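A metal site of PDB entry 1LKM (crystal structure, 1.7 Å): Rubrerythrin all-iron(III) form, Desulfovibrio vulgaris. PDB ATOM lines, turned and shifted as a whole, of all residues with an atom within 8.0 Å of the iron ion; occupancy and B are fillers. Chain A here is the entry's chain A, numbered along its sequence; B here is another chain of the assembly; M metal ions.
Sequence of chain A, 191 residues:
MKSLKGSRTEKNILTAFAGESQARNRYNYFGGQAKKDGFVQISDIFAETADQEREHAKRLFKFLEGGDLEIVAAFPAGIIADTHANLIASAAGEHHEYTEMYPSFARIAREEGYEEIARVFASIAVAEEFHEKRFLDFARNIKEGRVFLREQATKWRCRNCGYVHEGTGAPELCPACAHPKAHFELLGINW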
ATOM      1  N   ARG A 157     -15.337  17.324  32.712  1.00  0.00           N
ATOM      2  CA  ARG A 157     -14.252  17.962  31.976  1.00  0.00           C
ATOM      3  C   ARG A 157     -13.577  16.974  31.041  1.00  0.00           C
ATOM      4  O   ARG A 157     -13.337  15.827  31.403  1.00  0.00           O
ATOM      5  CB  ARG A 157     -13.203  18.521  32.940  1.00  0.00           C
ATOM      6  CG  ARG A 157     -12.132  19.372  32.245  1.00  0.00           C
ATOM      7  CD  ARG A 157     -11.020  19.799  33.194  1.00  0.00           C
ATOM      8  NE  ARG A 157     -10.151  18.682  33.562  1.00  0.00           N
ATOM      9  CZ  ARG A 157      -8.843  18.634  33.334  1.00  0.00           C
ATOM     10  NH1 ARG A 157      -8.234  19.647  32.742  1.00  0.00           N
ATOM     11  NH2 ARG A 157      -8.142  17.566  33.704  1.00  0.00           N
ATOM     12  N   CYS A 158     -13.272  17.430  29.820  1.00  0.00           N
ATOM     13  CA  CYS A 158     -12.580  16.601  28.856  1.00  0.00           C
ATOM     14  C   CYS A 158     -11.094  16.695  29.209  1.00  0.00           C
ATOM     15  O   CYS A 158     -10.531  17.783  29.232  1.00  0.00           O
ATOM     16  CB  CYS A 158     -12.804  17.125  27.434  1.00  0.00           C
ATOM     17  SG  CYS A 158     -11.837  16.230  26.197  1.00  0.00           S
ATOM     18  N   ARG A 159     -10.462  15.559  29.507  1.00  0.00           N
ATOM     19  CA  ARG A 159      -9.048  15.580  29.852  1.00  0.00           C
ATOM     20  C   ARG A 159      -8.166  15.906  28.656  1.00  0.00           C
ATOM     21  O   ARG A 159      -7.047  16.402  28.820  1.00  0.00           O
ATOM     22  CB  ARG A 159      -8.627  14.235  30.454  1.00  0.00           C
ATOM     23  CG  ARG A 159      -9.173  13.972  31.855  1.00  0.00           C
ATOM     24  CD  ARG A 159      -8.692  12.644  32.408  1.00  0.00           C
ATOM     25  NE  ARG A 159      -7.236  12.588  32.543  1.00  0.00           N
ATOM     26  CZ  ARG A 159      -6.540  13.234  33.465  1.00  0.00           C
ATOM     27  NH1 ARG A 159      -7.147  13.991  34.368  1.00  0.00           N
ATOM     28  NH2 ARG A 159      -5.209  13.130  33.485  1.00  0.00           N
ATOM     29  N   ASN A 160      -8.677  15.664  27.448  1.00  0.00           N
ATOM     30  CA  ASN A 160      -7.897  15.927  26.251  1.00  0.00           C
ATOM     31  C   ASN A 160      -7.772  17.407  25.884  1.00  0.00           C
ATOM     32  O   ASN A 160      -6.676  17.859  25.517  1.00  0.00           O
ATOM     33  CB  ASN A 160      -8.510  15.168  25.053  1.00  0.00           C
ATOM     34  CG  ASN A 160      -7.622  15.215  23.815  1.00  0.00           C
ATOM     35  OD1 ASN A 160      -8.019  15.712  22.766  1.00  0.00           O
ATOM     36  ND2 ASN A 160      -6.408  14.689  23.949  1.00  0.00           N
ATOM     37  N   CYS A 161      -8.857  18.170  26.005  1.00  0.00           N
ATOM     38  CA  CYS A 161      -8.828  19.585  25.631  1.00  0.00           C
ATOM     39  C   CYS A 161      -9.313  20.586  26.679  1.00  0.00           C
ATOM     40  O   CYS A 161      -9.153  21.797  26.483  1.00  0.00           O
ATOM     41  CB  CYS A 161      -9.624  19.794  24.345  1.00  0.00           C
ATOM     42  SG  CYS A 161     -11.419  19.750  24.555  1.00  0.00           S
ATOM     43  N   GLY A 162      -9.922  20.102  27.752  1.00  0.00           N
ATOM     44  CA  GLY A 162     -10.393  21.001  28.793  1.00  0.00           C
ATOM     45  C   GLY A 162     -11.842  21.441  28.670  1.00  0.00           C
ATOM     46  O   GLY A 162     -12.322  22.229  29.485  1.00  0.00           O
ATOM     47  N   TYR A 163     -12.546  20.953  27.655  1.00  0.00           N
ATOM     48  CA  TYR A 163     -13.947  21.332  27.501  1.00  0.00           C
ATOM     49  C   TYR A 163     -14.747  20.928  28.733  1.00  0.00           C
ATOM     50  O   TYR A 163     -14.509  19.874  29.315  1.00  0.00           O
ATOM     51  CB  TYR A 163     -14.549  20.651  26.267  1.00  0.00           C
ATOM     52  CG  TYR A 163     -16.015  20.984  26.070  1.00  0.00           C
ATOM     53  CD1 TYR A 163     -16.403  22.231  25.599  1.00  0.00           C
ATOM     54  CD2 TYR A 163     -17.008  20.058  26.402  1.00  0.00           C
ATOM     55  CE1 TYR A 163     -17.758  22.565  25.471  1.00  0.00           C
ATOM     56  CE2 TYR A 163     -18.351  20.374  26.280  1.00  0.00           C
ATOM     57  CZ  TYR A 163     -18.719  21.629  25.814  1.00  0.00           C
ATOM     58  OH  TYR A 163     -20.057  21.950  25.680  1.00  0.00           O
ATOM     59  N   VAL A 164     -15.687  21.788  29.137  1.00  0.00           N
ATOM     60  CA  VAL A 164     -16.531  21.508  30.296  1.00  0.00           C
ATOM     61  C   VAL A 164     -17.966  21.284  29.830  1.00  0.00           C
ATOM     62  O   VAL A 164     -18.547  22.130  29.159  1.00  0.00           O
ATOM     63  CB  VAL A 164     -16.492  22.663  31.314  1.00  0.00           C
ATOM     64  CG1 VAL A 164     -17.450  22.377  32.467  1.00  0.00           C
ATOM     65  CG2 VAL A 164     -15.076  22.850  31.839  1.00  0.00           C
ATOM     66  N   LEU A 173     -19.229  12.302  22.518  1.00  0.00           N
ATOM     67  CA  LEU A 173     -18.105  12.934  21.832  1.00  0.00           C
ATOM     68  C   LEU A 173     -17.910  14.344  22.363  1.00  0.00           C
ATOM     69  O   LEU A 173     -18.871  15.060  22.606  1.00  0.00           O
ATOM     70  CB  LEU A 173     -18.370  13.010  20.319  1.00  0.00           C
ATOM     71  CG  LEU A 173     -18.371  11.718  19.501  1.00  0.00           C
ATOM     72  CD1 LEU A 173     -18.750  12.040  18.057  1.00  0.00           C
ATOM     73  CD2 LEU A 173     -17.005  11.066  19.564  1.00  0.00           C
ATOM     74  N   CYS A 174     -16.652  14.735  22.561  1.00  0.00           N
ATOM     75  CA  CYS A 174     -16.383  16.090  23.042  1.00  0.00           C
ATOM     76  C   CYS A 174     -16.704  17.038  21.897  1.00  0.00           C
ATOM     77  O   CYS A 174     -16.189  16.890  20.792  1.00  0.00           O
ATOM     78  CB  CYS A 174     -14.908  16.241  23.425  1.00  0.00           C
ATOM     79  SG  CYS A 174     -14.489  17.926  23.935  1.00  0.00           S
ATOM     80  N   PRO A 175     -17.579  18.038  22.142  1.00  0.00           N
ATOM     81  CA  PRO A 175     -17.909  18.975  21.072  1.00  0.00           C
ATOM     82  C   PRO A 175     -16.754  19.860  20.628  1.00  0.00           C
ATOM     83  O   PRO A 175     -16.785  20.438  19.550  1.00  0.00           O
ATOM     84  CB  PRO A 175     -19.075  19.777  21.665  1.00  0.00           C
ATOM     85  CG  PRO A 175     -18.788  19.761  23.114  1.00  0.00           C
ATOM     86  CD  PRO A 175     -18.344  18.337  23.368  1.00  0.00           C
ATOM     87  N   ALA A 176     -15.718  19.961  21.459  1.00  0.00           N
ATOM     88  CA  ALA A 176     -14.559  20.780  21.112  1.00  0.00           C
ATOM     89  C   ALA A 176     -13.486  20.005  20.345  1.00  0.00           C
ATOM     90  O   ALA A 176     -13.136  20.374  19.231  1.00  0.00           O
ATOM     91  CB  ALA A 176     -13.950  21.399  22.380  1.00  0.00           C
ATOM     92  N   CYS A 177     -12.981  18.915  20.926  1.00  0.00           N
ATOM     93  CA  CYS A 177     -11.917  18.138  20.280  1.00  0.00           C
ATOM     94  C   CYS A 177     -12.342  16.832  19.603  1.00  0.00           C
ATOM     95  O   CYS A 177     -11.495  16.113  19.060  1.00  0.00           O
ATOM     96  CB  CYS A 177     -10.802  17.827  21.280  1.00  0.00           C
ATOM     97  SG  CYS A 177     -11.249  16.591  22.506  1.00  0.00           S
ATOM     98  N   ALA A 178     -13.637  16.530  19.634  1.00  0.00           N
ATOM     99  CA  ALA A 178     -14.176  15.330  19.003  1.00  0.00           C
ATOM    100  C   ALA A 178     -13.675  14.010  19.561  1.00  0.00           C
ATOM    101  O   ALA A 178     -13.868  12.955  18.949  1.00  0.00           O
ATOM    102  CB  ALA A 178     -13.938  15.380  17.495  1.00  0.00           C
ATOM    103  N   HIS A 179     -13.021  14.040  20.721  1.00  0.00           N
ATOM    104  CA  HIS A 179     -12.554  12.791  21.321  1.00  0.00           C
ATOM    105  C   HIS A 179     -13.719  12.113  22.027  1.00  0.00           C
ATOM    106  O   HIS A 179     -14.682  12.772  22.437  1.00  0.00           O
ATOM    107  CB  HIS A 179     -11.385  13.042  22.268  1.00  0.00           C
ATOM    108  CG  HIS A 179     -10.066  13.156  21.577  1.00  0.00           C
ATOM    109  ND1 HIS A 179      -9.832  14.071  20.569  1.00  0.00           N
ATOM    110  CD2 HIS A 179      -8.927  12.431  21.703  1.00  0.00           C
ATOM    111  CE1 HIS A 179      -8.611  13.899  20.107  1.00  0.00           C
ATOM    112  NE2 HIS A 179      -8.036  12.914  20.778  1.00  0.00           N
ATOM    113  N   PRO A 180     -13.668  10.779  22.155  1.00  0.00           N
ATOM    114  CA  PRO A 180     -14.730  10.014  22.809  1.00  0.00           C
ATOM    115  C   PRO A 180     -14.927  10.248  24.298  1.00  0.00           C
ATOM    116  O   PRO A 180     -14.048  10.764  24.993  1.00  0.00           O
ATOM    117  CB  PRO A 180     -14.358   8.569  22.494  1.00  0.00           C
ATOM    118  CG  PRO A 180     -12.877   8.608  22.490  1.00  0.00           C
ATOM    119  CD  PRO A 180     -12.592   9.881  21.705  1.00  0.00           C
ATOM    120  N   HIS A 183     -12.554  10.184  27.547  1.00  0.00           N
ATOM    121  CA  HIS A 183     -11.677  11.227  28.052  1.00  0.00           C
ATOM    122  C   HIS A 183     -12.256  12.103  29.167  1.00  0.00           C
ATOM    123  O   HIS A 183     -11.531  12.892  29.771  1.00  0.00           O
ATOM    124  CB  HIS A 183     -11.213  12.116  26.893  1.00  0.00           C
ATOM    125  CG  HIS A 183     -10.300  11.406  25.937  1.00  0.00           C
ATOM    126  ND1 HIS A 183      -8.923  11.481  26.035  1.00  0.00           N
ATOM    127  CD2 HIS A 183     -10.563  10.564  24.907  1.00  0.00           C
ATOM    128  CE1 HIS A 183      -8.385  10.703  25.107  1.00  0.00           C
ATOM    129  NE2 HIS A 183      -9.356  10.143  24.417  1.00  0.00           N
ATOM    130  N   PHE A 184     -13.545  11.967  29.445  1.00  0.00           N
ATOM    131  CA  PHE A 184     -14.175  12.792  30.470  1.00  0.00           C
ATOM    132  C   PHE A 184     -14.061  12.319  31.915  1.00  0.00           C
ATOM    133  O   PHE A 184     -13.976  11.133  32.203  1.00  0.00           O
ATOM    134  CB  PHE A 184     -15.657  13.002  30.140  1.00  0.00           C
ATOM    135  CG  PHE A 184     -15.894  13.967  29.009  1.00  0.00           C
ATOM    136  CD1 PHE A 184     -15.863  13.522  27.683  1.00  0.00           C
ATOM    137  CD2 PHE A 184     -16.119  15.318  29.265  1.00  0.00           C
ATOM    138  CE1 PHE A 184     -16.055  14.428  26.630  1.00  0.00           C
ATOM    139  CE2 PHE A 184     -16.317  16.219  28.224  1.00  0.00           C
ATOM    140  CZ  PHE A 184     -16.286  15.774  26.898  1.00  0.00           C
ATOM    141  N   GLN B  52      -3.446  20.725  26.142  1.00  0.00           N
ATOM    142  CA  GLN B  52      -4.821  20.913  25.692  1.00  0.00           C
ATOM    143  C   GLN B  52      -4.846  21.934  24.551  1.00  0.00           C
ATOM    144  O   GLN B  52      -5.663  21.805  23.640  1.00  0.00           O
ATOM    145  CB  GLN B  52      -5.717  21.314  26.878  1.00  0.00           C
ATOM    146  CG  GLN B  52      -5.662  20.246  27.978  1.00  0.00           C
ATOM    147  CD  GLN B  52      -6.650  20.445  29.104  1.00  0.00           C
ATOM    148  OE1 GLN B  52      -6.938  21.574  29.507  1.00  0.00           O
ATOM    149  NE2 GLN B  52      -7.170  19.344  29.646  1.00  0.00           N
ATOM    150  N   GLU B  55      -4.248  20.213  21.445  1.00  0.00           N
ATOM    151  CA  GLU B  55      -5.434  19.541  20.932  1.00  0.00           C
ATOM    152  C   GLU B  55      -6.431  20.510  20.275  1.00  0.00           C
ATOM    153  O   GLU B  55      -7.062  20.161  19.274  1.00  0.00           O
ATOM    154  CB  GLU B  55      -6.098  18.740  22.053  1.00  0.00           C
ATOM    155  CG  GLU B  55      -5.196  17.607  22.581  1.00  0.00           C
ATOM    156  CD  GLU B  55      -4.799  16.635  21.480  1.00  0.00           C
ATOM    157  OE1 GLU B  55      -5.699  16.178  20.752  1.00  0.00           O
ATOM    158  OE2 GLU B  55      -3.605  16.320  21.355  1.00  0.00           O
ATOM    159  N   HIS B  56      -6.581  21.706  20.816  1.00  0.00           N
ATOM    160  CA  HIS B  56      -7.471  22.684  20.188  1.00  0.00           C
ATOM    161  C   HIS B  56      -6.874  22.990  18.815  1.00  0.00           C
ATOM    162  O   HIS B  56      -7.586  23.063  17.802  1.00  0.00           O
ATOM    163  CB  HIS B  56      -7.520  23.978  21.008  1.00  0.00           C
ATOM    164  CG  HIS B  56      -8.280  23.844  22.291  1.00  0.00           C
ATOM    165  ND1 HIS B  56      -8.033  24.641  23.386  1.00  0.00           N
ATOM    166  CD2 HIS B  56      -9.274  23.000  22.653  1.00  0.00           C
ATOM    167  CE1 HIS B  56      -8.840  24.287  24.376  1.00  0.00           C
ATOM    168  NE2 HIS B  56      -9.601  23.297  23.958  1.00  0.00           N
ATOM    169  N   ARG B  59      -7.531  20.150  16.227  1.00  0.00           N
ATOM    170  CA  ARG B  59      -8.891  20.175  15.700  1.00  0.00           C
ATOM    171  C   ARG B  59      -8.989  21.251  14.626  1.00  0.00           C
ATOM    172  O   ARG B  59      -9.573  21.043  13.560  1.00  0.00           O
ATOM    173  CB  ARG B  59      -9.904  20.465  16.822  1.00  0.00           C
ATOM    174  CG  ARG B  59     -11.373  20.371  16.376  1.00  0.00           C
ATOM    175  CD  ARG B  59     -11.732  18.951  15.990  1.00  0.00           C
ATOM    176  NE  ARG B  59     -12.998  18.831  15.263  1.00  0.00           N
ATOM    177  CZ  ARG B  59     -14.207  18.858  15.815  1.00  0.00           C
ATOM    178  NH1 ARG B  59     -14.337  19.008  17.128  1.00  0.00           N
ATOM    179  NH2 ARG B  59     -15.289  18.714  15.062  1.00  0.00           N
ATOM    180  N   SER B 123     -17.268  25.863  21.254  1.00  0.00           N
ATOM    181  CA  SER B 123     -16.966  24.830  22.232  1.00  0.00           C
ATOM    182  C   SER B 123     -15.571  25.032  22.821  1.00  0.00           C
ATOM    183  O   SER B 123     -15.374  24.871  24.025  1.00  0.00           O
ATOM    184  CB  SER B 123     -17.078  23.451  21.592  1.00  0.00           C
ATOM    185  OG  SER B 123     -18.425  23.177  21.238  1.00  0.00           O
ATOM    186  N   ALA B 127     -13.708  25.723  27.025  1.00  0.00           N
ATOM    187  CA  ALA B 127     -12.504  25.177  27.644  1.00  0.00           C
ATOM    188  C   ALA B 127     -11.591  26.311  28.090  1.00  0.00           C
ATOM    189  O   ALA B 127     -11.002  26.257  29.172  1.00  0.00           O
ATOM    190  CB  ALA B 127     -11.768  24.273  26.666  1.00  0.00           C
HETATM  191 FE    FE M   1     -12.199  17.636  24.338  1.00  0.00          FE
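The iron ion is bound by the side-chain sulfur (SG) of Cys 161. The iron ion is bound by SG of Cys 177, 2.3 Å away. The iron ion is bound by SG of Cys 174, 2.3 Å away. The iron ion is bound by SG of Cys 158 (2.4 Å). The iron ion has four donor atoms within binding distance.
Four residues have an atom within 4 Å of the iron ion: Cys 158, Cys 161, Cys 174 and Cys 177.
NE2 of His 56 of chain B lies within hydrogen-bond range of O of Cys 161, at 3.0 Å. The backbone NH of Cys 158 lies within hydrogen-bond range of the backbone carbonyl oxygen of Tyr 163, at 2.8 Å. O of Cys 177 is in hydrogen-bond range of ND1 of His 179 (3.0 Å). N of Tyr 163 lies close to SG of Cys 161. The side-chain sulfur of Cys 174 sits close to the backbone NH of Ala 176, 3.4 Å away. O of His 179 sits at hydrogen-bond distance from N of Cys 174 (2.8 Å). The backbone NH (N) of Asn 160 sits close to the side-chain sulfur (SG) of Cys 158 (3.4 Å). OD1 of Asn 160 lies close to SG of Cys 177 (3.4 Å).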
